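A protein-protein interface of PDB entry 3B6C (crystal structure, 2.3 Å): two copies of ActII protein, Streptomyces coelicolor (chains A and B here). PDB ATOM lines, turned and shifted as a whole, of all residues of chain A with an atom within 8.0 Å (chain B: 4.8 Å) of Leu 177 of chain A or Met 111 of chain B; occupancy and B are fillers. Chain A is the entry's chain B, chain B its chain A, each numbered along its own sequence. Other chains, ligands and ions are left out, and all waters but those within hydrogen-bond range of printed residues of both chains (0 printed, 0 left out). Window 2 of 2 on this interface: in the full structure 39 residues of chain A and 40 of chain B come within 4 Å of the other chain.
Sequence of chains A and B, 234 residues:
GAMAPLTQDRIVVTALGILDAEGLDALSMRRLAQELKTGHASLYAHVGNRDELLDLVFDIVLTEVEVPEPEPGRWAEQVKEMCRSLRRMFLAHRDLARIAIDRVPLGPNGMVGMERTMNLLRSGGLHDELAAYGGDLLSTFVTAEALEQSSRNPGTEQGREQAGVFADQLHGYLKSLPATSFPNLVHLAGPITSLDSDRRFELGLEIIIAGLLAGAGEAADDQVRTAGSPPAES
The side-chain carboxylate of Glu 115 of chain B lies close to the backbone nitrogen of Pro 183 of chain A (3.5 Å).
OE1 of Glu 115 of chain B is in hydrogen-bond range of N of Leu 185 of chain A, at 3.0 Å.
The side-chain carboxylate (OE2) of Glu 115 of chain B is in hydrogen-bond range of the side-chain amide nitrogen (ND2) of Asn 184 of chain A, 2.6 Å away.
Among the printed residues, merely in contact across the chains: Leu 170 of chain A with Leu 106 of chain B (3.0 Å), Phe 182 of chain A with Glu 115 of chain B (3.1 Å), Leu 185 of chain A with Met 111 of chain B (3.7 Å), Leu 185 of chain A with Met 114 of chain B (3.7 Å), Ser 181 of chain A with Glu 115 of chain B (3.97 Å), Phe 182 of chain A with Met 111 of chain B (3.98 Å), Tyr 173 of chain A with Met 111 of chain B (3.98 Å) and Leu 177 of chain A with Met 111 of chain B (3.98 Å).
Of the printed residues of chain B, Leu 177 of chain A touches Met 111 (3.98 Å).
Of the printed residues of chain A, Met 111 of chain B touches Tyr 173 (3.98 Å), Leu 177 (3.98 Å), Phe 182 (3.98 Å) and Leu 185 (3.7 Å).
Gly 110 of chain B touches none of the printed residues of chain A.
Of the printed residues of chain B, Tyr 173 of chain A touches Met 111 (3.98 Å).
Printed residues of chain B within 4 Å of Leu 170 of chain A: Leu 106 (3.0 Å).
Of the printed residues of chain A, Leu 106 of chain B touches Leu 170.
Printed residues of chain B within 4 Å of Phe 182 of chain A: Met 111 (3.98 Å) and Glu 115 (3.1 Å).
Of the printed residues of chain B, Asn 184 of chain A touches Glu 115.
Gly 113 of chain B touches none of the printed residues of chain A.
Val 186 of chain A touches none of the printed residues of chain B.
The nearest printed residue of chain B that does not touch Leu 177 of chain A is Leu 106 of chain B (6.7 Å).
The nearest printed residue of chain A that does not touch Met 111 of chain B is Leu 174 of chain A (5.1 Å).
The nearest printed residue of chain A that does not touch Met 114 of chain B is Leu 174 of chain A (5.3 Å).
Printed residues of chain B that touch a printed residue of chain A: Leu 106, Met 111, Met 114 and Glu 115.
Hydrophobic or aromatic side chains of chain B that line the printed part of chain A: Leu 106 and Met 111.
Along chain B the printed residues that touch a printed residue of chain A span positions 106 to 115.
Hydrophobic or aromatic side chains of chain A within 4 Å of the printed part of chain B: Leu 170, Tyr 173, Leu 177, Phe 182, Pro 183 and Leu 185.
Among the printed residues, no Asp or Glu carboxylate lies within 4 Å of a Lys or Arg side-chain nitrogen of the other chain.
No position is printed for both chains.
Of the 11 pairs that touch across the chains among the printed residues, none has its exchanged pair printed and touching as well.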
ATOM      1  N   LEU A 170     -26.940 -15.947  10.250  1.00  0.00           N
ATOM      2  CA  LEU A 170     -26.463 -14.923  11.177  1.00  0.00           C
ATOM      3  C   LEU A 170     -26.488 -15.480  12.607  1.00  0.00           C
ATOM      4  O   LEU A 170     -25.514 -15.353  13.344  1.00  0.00           O
ATOM      5  CB  LEU A 170     -27.348 -13.677  11.102  1.00  0.00           C
ATOM      6  CG  LEU A 170     -26.711 -12.362  11.578  1.00  0.00           C
ATOM      7  CD1 LEU A 170     -27.509 -11.780  12.732  1.00  0.00           C
ATOM      8  CD2 LEU A 170     -25.264 -12.597  11.988  1.00  0.00           C
ATOM      9  N   HIS A 171     -27.603 -16.097  12.988  1.00  0.00           N
ATOM     10  CA  HIS A 171     -27.744 -16.673  14.321  1.00  0.00           C
ATOM     11  C   HIS A 171     -26.573 -17.611  14.633  1.00  0.00           C
ATOM     12  O   HIS A 171     -26.018 -17.580  15.734  1.00  0.00           O
ATOM     13  CB  HIS A 171     -29.065 -17.448  14.429  1.00  0.00           C
ATOM     14  CG  HIS A 171     -29.213 -18.212  15.706  1.00  0.00           C
ATOM     15  ND1 HIS A 171     -28.146 -18.491  16.534  1.00  0.00           N
ATOM     16  CD2 HIS A 171     -30.296 -18.774  16.290  1.00  0.00           C
ATOM     17  CE1 HIS A 171     -28.564 -19.190  17.574  1.00  0.00           C
ATOM     18  NE2 HIS A 171     -29.865 -19.375  17.449  1.00  0.00           N
ATOM     19  N   GLY A 172     -26.210 -18.445  13.659  1.00  0.00           N
ATOM     20  CA  GLY A 172     -25.106 -19.380  13.828  1.00  0.00           C
ATOM     21  C   GLY A 172     -23.764 -18.668  13.814  1.00  0.00           C
ATOM     22  O   GLY A 172     -22.844 -19.039  14.553  1.00  0.00           O
ATOM     23  N   TYR A 173     -23.643 -17.663  12.949  1.00  0.00           N
ATOM     24  CA  TYR A 173     -22.421 -16.876  12.866  1.00  0.00           C
ATOM     25  C   TYR A 173     -22.041 -16.361  14.261  1.00  0.00           C
ATOM     26  O   TYR A 173     -20.881 -16.452  14.670  1.00  0.00           O
ATOM     27  CB  TYR A 173     -22.630 -15.688  11.932  1.00  0.00           C
ATOM     28  CG  TYR A 173     -21.423 -14.788  11.802  1.00  0.00           C
ATOM     29  CD1 TYR A 173     -21.169 -13.788  12.737  1.00  0.00           C
ATOM     30  CD2 TYR A 173     -20.531 -14.940  10.743  1.00  0.00           C
ATOM     31  CE1 TYR A 173     -20.055 -12.967  12.624  1.00  0.00           C
ATOM     32  CE2 TYR A 173     -19.417 -14.122  10.621  1.00  0.00           C
ATOM     33  CZ  TYR A 173     -19.185 -13.140  11.563  1.00  0.00           C
ATOM     34  OH  TYR A 173     -18.084 -12.331  11.446  1.00  0.00           O
ATOM     35  N   LEU A 174     -23.022 -15.834  14.994  1.00  0.00           N
ATOM     36  CA  LEU A 174     -22.771 -15.307  16.324  1.00  0.00           C
ATOM     37  C   LEU A 174     -22.446 -16.390  17.345  1.00  0.00           C
ATOM     38  O   LEU A 174     -21.574 -16.209  18.190  1.00  0.00           O
ATOM     39  CB  LEU A 174     -23.973 -14.478  16.787  1.00  0.00           C
ATOM     40  CG  LEU A 174     -24.258 -13.288  15.868  1.00  0.00           C
ATOM     41  CD1 LEU A 174     -25.463 -12.526  16.376  1.00  0.00           C
ATOM     42  CD2 LEU A 174     -23.049 -12.375  15.804  1.00  0.00           C
ATOM     43  N   LYS A 175     -23.129 -17.521  17.254  1.00  0.00           N
ATOM     44  CA  LYS A 175     -22.901 -18.618  18.184  1.00  0.00           C
ATOM     45  C   LYS A 175     -21.469 -19.132  18.113  1.00  0.00           C
ATOM     46  O   LYS A 175     -20.956 -19.704  19.080  1.00  0.00           O
ATOM     47  CB  LYS A 175     -23.857 -19.783  17.855  1.00  0.00           C
ATOM     48  N   SER A 176     -20.827 -18.928  16.967  1.00  0.00           N
ATOM     49  CA  SER A 176     -19.510 -19.501  16.715  1.00  0.00           C
ATOM     50  C   SER A 176     -18.406 -18.619  17.293  1.00  0.00           C
ATOM     51  O   SER A 176     -17.255 -19.042  17.402  1.00  0.00           O
ATOM     52  CB  SER A 176     -19.291 -19.700  15.214  1.00  0.00           C
ATOM     53  OG  SER A 176     -20.411 -20.329  14.615  1.00  0.00           O
ATOM     54  N   LEU A 177     -18.765 -17.395  17.661  1.00  0.00           N
ATOM     55  CA  LEU A 177     -17.788 -16.412  18.111  1.00  0.00           C
ATOM     56  C   LEU A 177     -16.916 -16.973  19.229  1.00  0.00           C
ATOM     57  O   LEU A 177     -17.366 -17.796  20.026  1.00  0.00           O
ATOM     58  CB  LEU A 177     -18.488 -15.135  18.580  1.00  0.00           C
ATOM     59  CG  LEU A 177     -18.611 -14.011  17.549  1.00  0.00           C
ATOM     60  CD1 LEU A 177     -17.832 -14.351  16.288  1.00  0.00           C
ATOM     61  CD2 LEU A 177     -20.072 -13.737  17.225  1.00  0.00           C
ATOM     62  N   PRO A 178     -15.667 -16.521  19.282  1.00  0.00           N
ATOM     63  CA  PRO A 178     -14.791 -16.813  20.421  1.00  0.00           C
ATOM     64  C   PRO A 178     -15.413 -16.372  21.742  1.00  0.00           C
ATOM     65  O   PRO A 178     -15.284 -15.209  22.125  1.00  0.00           O
ATOM     66  CB  PRO A 178     -13.545 -15.976  20.120  1.00  0.00           C
ATOM     67  CG  PRO A 178     -13.522 -15.867  18.638  1.00  0.00           C
ATOM     68  CD  PRO A 178     -14.961 -15.803  18.208  1.00  0.00           C
ATOM     69  N   ALA A 179     -16.079 -17.296  22.425  1.00  0.00           N
ATOM     70  CA  ALA A 179     -16.885 -16.954  23.591  1.00  0.00           C
ATOM     71  C   ALA A 179     -16.058 -16.208  24.634  1.00  0.00           C
ATOM     72  O   ALA A 179     -16.602 -15.650  25.587  1.00  0.00           O
ATOM     73  CB  ALA A 179     -17.499 -18.207  24.197  1.00  0.00           C
ATOM     74  N   THR A 180     -14.743 -16.203  24.446  1.00  0.00           N
ATOM     75  CA  THR A 180     -13.834 -15.582  25.402  1.00  0.00           C
ATOM     76  C   THR A 180     -13.663 -14.094  25.113  1.00  0.00           C
ATOM     77  O   THR A 180     -13.310 -13.317  26.001  1.00  0.00           O
ATOM     78  CB  THR A 180     -12.454 -16.258  25.389  1.00  0.00           C
ATOM     79  OG1 THR A 180     -12.498 -17.422  24.555  1.00  0.00           O
ATOM     80  CG2 THR A 180     -12.047 -16.663  26.798  1.00  0.00           C
ATOM     81  N   SER A 181     -13.914 -13.706  23.867  1.00  0.00           N
ATOM     82  CA  SER A 181     -13.815 -12.320  23.470  1.00  0.00           C
ATOM     83  C   SER A 181     -15.211 -11.735  23.259  1.00  0.00           C
ATOM     84  O   SER A 181     -15.448 -10.584  23.591  1.00  0.00           O
ATOM     85  CB  SER A 181     -12.958 -12.204  22.205  1.00  0.00           C
ATOM     86  OG  SER A 181     -11.657 -12.724  22.434  1.00  0.00           O
ATOM     87  N   PHE A 182     -16.128 -12.543  22.728  1.00  0.00           N
ATOM     88  CA  PHE A 182     -17.503 -12.101  22.489  1.00  0.00           C
ATOM     89  C   PHE A 182     -18.459 -12.915  23.321  1.00  0.00           C
ATOM     90  O   PHE A 182     -19.273 -13.688  22.809  1.00  0.00           O
ATOM     91  CB  PHE A 182     -17.823 -12.228  21.015  1.00  0.00           C
ATOM     92  CG  PHE A 182     -16.905 -11.445  20.162  1.00  0.00           C
ATOM     93  CD1 PHE A 182     -15.766 -12.024  19.619  1.00  0.00           C
ATOM     94  CD2 PHE A 182     -17.137 -10.099  19.962  1.00  0.00           C
ATOM     95  CE1 PHE A 182     -14.870 -11.263  18.888  1.00  0.00           C
ATOM     96  CE2 PHE A 182     -16.254  -9.329  19.235  1.00  0.00           C
ATOM     97  CZ  PHE A 182     -15.117  -9.907  18.697  1.00  0.00           C
ATOM     98  N   PRO A 183     -18.362 -12.761  24.642  1.00  0.00           N
ATOM     99  CA  PRO A 183     -19.209 -13.502  25.580  1.00  0.00           C
ATOM    100  C   PRO A 183     -20.693 -13.200  25.449  1.00  0.00           C
ATOM    101  O   PRO A 183     -21.520 -14.105  25.279  1.00  0.00           O
ATOM    102  CB  PRO A 183     -18.640 -13.120  26.947  1.00  0.00           C
ATOM    103  CG  PRO A 183     -18.011 -11.789  26.727  1.00  0.00           C
ATOM    104  CD  PRO A 183     -17.443 -11.837  25.338  1.00  0.00           C
ATOM    105  N   ASN A 184     -21.046 -11.920  25.523  1.00  0.00           N
ATOM    106  CA  ASN A 184     -22.451 -11.531  25.422  1.00  0.00           C
ATOM    107  C   ASN A 184     -23.080 -11.943  24.106  1.00  0.00           C
ATOM    108  O   ASN A 184     -24.187 -12.471  24.098  1.00  0.00           O
ATOM    109  CB  ASN A 184     -22.585 -10.028  25.603  1.00  0.00           C
ATOM    110  CG  ASN A 184     -22.145  -9.575  26.978  1.00  0.00           C
ATOM    111  OD1 ASN A 184     -22.925  -9.591  27.932  1.00  0.00           O
ATOM    112  ND2 ASN A 184     -20.882  -9.179  27.089  1.00  0.00           N
ATOM    113  N   LEU A 185     -22.369 -11.723  22.999  1.00  0.00           N
ATOM    114  CA  LEU A 185     -22.881 -12.062  21.678  1.00  0.00           C
ATOM    115  C   LEU A 185     -23.233 -13.532  21.546  1.00  0.00           C
ATOM    116  O   LEU A 185     -24.309 -13.866  21.063  1.00  0.00           O
ATOM    117  CB  LEU A 185     -21.870 -11.668  20.602  1.00  0.00           C
ATOM    118  CG  LEU A 185     -22.076 -10.374  19.813  1.00  0.00           C
ATOM    119  CD1 LEU A 185     -22.660  -9.256  20.656  1.00  0.00           C
ATOM    120  CD2 LEU A 185     -20.731  -9.974  19.236  1.00  0.00           C
ATOM    121  N   VAL A 186     -22.340 -14.418  21.978  1.00  0.00           N
ATOM    122  CA  VAL A 186     -22.622 -15.847  21.884  1.00  0.00           C
ATOM    123  C   VAL A 186     -23.801 -16.218  22.757  1.00  0.00           C
ATOM    124  O   VAL A 186     -24.676 -16.983  22.349  1.00  0.00           O
ATOM    125  CB  VAL A 186     -21.448 -16.715  22.341  1.00  0.00           C
ATOM    126  CG1 VAL A 186     -21.713 -18.170  21.951  1.00  0.00           C
ATOM    127  CG2 VAL A 186     -20.159 -16.214  21.735  1.00  0.00           C
ATOM    128  N   HIS A 187     -23.825 -15.679  23.969  1.00  0.00           N
ATOM    129  CA  HIS A 187     -24.916 -15.987  24.876  1.00  0.00           C
ATOM    130  C   HIS A 187     -26.248 -15.368  24.467  1.00  0.00           C
ATOM    131  O   HIS A 187     -27.304 -15.831  24.904  1.00  0.00           O
ATOM    132  CB  HIS A 187     -24.569 -15.564  26.308  1.00  0.00           C
ATOM    133  CG  HIS A 187     -25.712 -15.697  27.270  1.00  0.00           C
ATOM    134  ND1 HIS A 187     -25.621 -16.406  28.447  1.00  0.00           N
ATOM    135  CD2 HIS A 187     -26.980 -15.221  27.216  1.00  0.00           C
ATOM    136  CE1 HIS A 187     -26.783 -16.367  29.075  1.00  0.00           C
ATOM    137  NE2 HIS A 187     -27.624 -15.655  28.348  1.00  0.00           N
ATOM    138  N   ALA A 189     -26.955 -14.806  21.122  1.00  0.00           N
ATOM    139  CA  ALA A 189     -27.093 -15.067  19.696  1.00  0.00           C
ATOM    140  C   ALA A 189     -28.532 -15.328  19.237  1.00  0.00           C
ATOM    141  O   ALA A 189     -28.957 -14.817  18.202  1.00  0.00           O
ATOM    142  CB  ALA A 189     -26.185 -16.223  19.296  1.00  0.00           C
ATOM    143  N   PRO B 105     -24.689  -3.995  11.039  1.00  0.00           N
ATOM    144  CA  PRO B 105     -23.435  -3.476  11.595  1.00  0.00           C
ATOM    145  C   PRO B 105     -22.317  -4.514  11.562  1.00  0.00           C
ATOM    146  O   PRO B 105     -21.184  -4.184  11.210  1.00  0.00           O
ATOM    147  CB  PRO B 105     -23.806  -3.147  13.042  1.00  0.00           C
ATOM    148  CG  PRO B 105     -24.941  -4.055  13.354  1.00  0.00           C
ATOM    149  CD  PRO B 105     -25.717  -4.190  12.077  1.00  0.00           C
ATOM    150  N   LEU B 106     -22.636  -5.751  11.925  1.00  0.00           N
ATOM    151  CA  LEU B 106     -21.651  -6.827  11.934  1.00  0.00           C
ATOM    152  C   LEU B 106     -20.384  -6.429  11.183  1.00  0.00           C
ATOM    153  O   LEU B 106     -20.441  -6.011  10.027  1.00  0.00           O
ATOM    154  CB  LEU B 106     -22.243  -8.100  11.327  1.00  0.00           C
ATOM    155  CG  LEU B 106     -23.299  -8.826  12.163  1.00  0.00           C
ATOM    156  CD1 LEU B 106     -23.522 -10.238  11.640  1.00  0.00           C
ATOM    157  CD2 LEU B 106     -22.900  -8.851  13.630  1.00  0.00           C
ATOM    158  N   GLY B 107     -19.243  -6.561  11.852  1.00  0.00           N
ATOM    159  CA  GLY B 107     -17.964  -6.217  11.259  1.00  0.00           C
ATOM    160  C   GLY B 107     -16.981  -5.691  12.286  1.00  0.00           C
ATOM    161  O   GLY B 107     -17.377  -5.098  13.290  1.00  0.00           O
ATOM    162  N   PRO B 108     -15.694  -5.907  12.034  1.00  0.00           N
ATOM    163  CA  PRO B 108     -14.645  -5.450  12.949  1.00  0.00           C
ATOM    164  C   PRO B 108     -15.224  -4.697  14.144  1.00  0.00           C
ATOM    165  O   PRO B 108     -15.493  -5.303  15.182  1.00  0.00           O
ATOM    166  CB  PRO B 108     -13.820  -4.500  12.080  1.00  0.00           C
ATOM    167  CG  PRO B 108     -13.990  -5.027  10.699  1.00  0.00           C
ATOM    168  CD  PRO B 108     -15.389  -5.578  10.631  1.00  0.00           C
ATOM    169  N   ASN B 109     -15.412  -3.390  13.992  1.00  0.00           N
ATOM    170  CA  ASN B 109     -15.960  -2.565  15.061  1.00  0.00           C
ATOM    171  C   ASN B 109     -17.456  -2.791  15.254  1.00  0.00           C
ATOM    172  O   ASN B 109     -17.970  -2.690  16.368  1.00  0.00           O
ATOM    173  CB  ASN B 109     -15.682  -1.085  14.792  1.00  0.00           C
ATOM    174  CG  ASN B 109     -14.423  -0.868  13.975  1.00  0.00           C
ATOM    175  OD1 ASN B 109     -13.313  -1.108  14.448  1.00  0.00           O
ATOM    176  ND2 ASN B 109     -14.591  -0.411  12.739  1.00  0.00           N
ATOM    177  N   GLY B 110     -18.149  -3.096  14.162  1.00  0.00           N
ATOM    178  CA  GLY B 110     -19.579  -3.335  14.208  1.00  0.00           C
ATOM    179  C   GLY B 110     -19.966  -4.343  15.273  1.00  0.00           C
ATOM    180  O   GLY B 110     -20.823  -4.074  16.114  1.00  0.00           O
ATOM    181  N   MET B 111     -19.329  -5.509  15.235  1.00  0.00           N
ATOM    182  CA  MET B 111     -19.607  -6.565  16.200  1.00  0.00           C
ATOM    183  C   MET B 111     -19.055  -6.214  17.577  1.00  0.00           C
ATOM    184  O   MET B 111     -19.689  -6.482  18.598  1.00  0.00           O
ATOM    185  CB  MET B 111     -19.022  -7.895  15.723  1.00  0.00           C
ATOM    186  CG  MET B 111     -17.503  -7.915  15.650  1.00  0.00           C
ATOM    187  SD  MET B 111     -16.853  -9.517  15.138  1.00  0.00           S
ATOM    188  CE  MET B 111     -18.321 -10.535  15.258  1.00  0.00           C
ATOM    189  N   VAL B 112     -17.870  -5.612  17.599  1.00  0.00           N
ATOM    190  CA  VAL B 112     -17.231  -5.223  18.851  1.00  0.00           C
ATOM    191  C   VAL B 112     -18.116  -4.274  19.652  1.00  0.00           C
ATOM    192  O   VAL B 112     -18.190  -4.362  20.876  1.00  0.00           O
ATOM    193  CB  VAL B 112     -15.867  -4.551  18.604  1.00  0.00           C
ATOM    194  CG1 VAL B 112     -15.359  -3.896  19.879  1.00  0.00           C
ATOM    195  CG2 VAL B 112     -14.862  -5.567  18.081  1.00  0.00           C
ATOM    196  N   GLY B 113     -18.788  -3.366  18.949  1.00  0.00           N
ATOM    197  CA  GLY B 113     -19.626  -2.373  19.593  1.00  0.00           C
ATOM    198  C   GLY B 113     -20.965  -2.937  20.027  1.00  0.00           C
ATOM    199  O   GLY B 113     -21.611  -2.405  20.930  1.00  0.00           O
ATOM    200  N   MET B 114     -21.383  -4.020  19.380  1.00  0.00           N
ATOM    201  CA  MET B 114     -22.550  -4.774  19.821  1.00  0.00           C
ATOM    202  C   MET B 114     -22.242  -5.583  21.077  1.00  0.00           C
ATOM    203  O   MET B 114     -22.999  -5.555  22.046  1.00  0.00           O
ATOM    204  CB  MET B 114     -23.043  -5.699  18.708  1.00  0.00           C
ATOM    205  CG  MET B 114     -24.521  -6.047  18.797  1.00  0.00           C
ATOM    206  SD  MET B 114     -24.999  -7.352  17.650  1.00  0.00           S
ATOM    207  CE  MET B 114     -24.083  -6.871  16.188  1.00  0.00           C
ATOM    208  N   GLU B 115     -21.126  -6.304  21.050  1.00  0.00           N
ATOM    209  CA  GLU B 115     -20.603  -6.950  22.247  1.00  0.00           C
ATOM    210  C   GLU B 115     -20.568  -5.984  23.426  1.00  0.00           C
ATOM    211  O   GLU B 115     -21.011  -6.315  24.526  1.00  0.00           O
ATOM    212  CB  GLU B 115     -19.203  -7.511  21.986  1.00  0.00           C
ATOM    213  CG  GLU B 115     -18.544  -8.131  23.207  1.00  0.00           C
ATOM    214  CD  GLU B 115     -19.316  -9.321  23.743  1.00  0.00           C
ATOM    215  OE1 GLU B 115     -19.836 -10.111  22.927  1.00  0.00           O
ATOM    216  OE2 GLU B 115     -19.403  -9.466  24.980  1.00  0.00           O
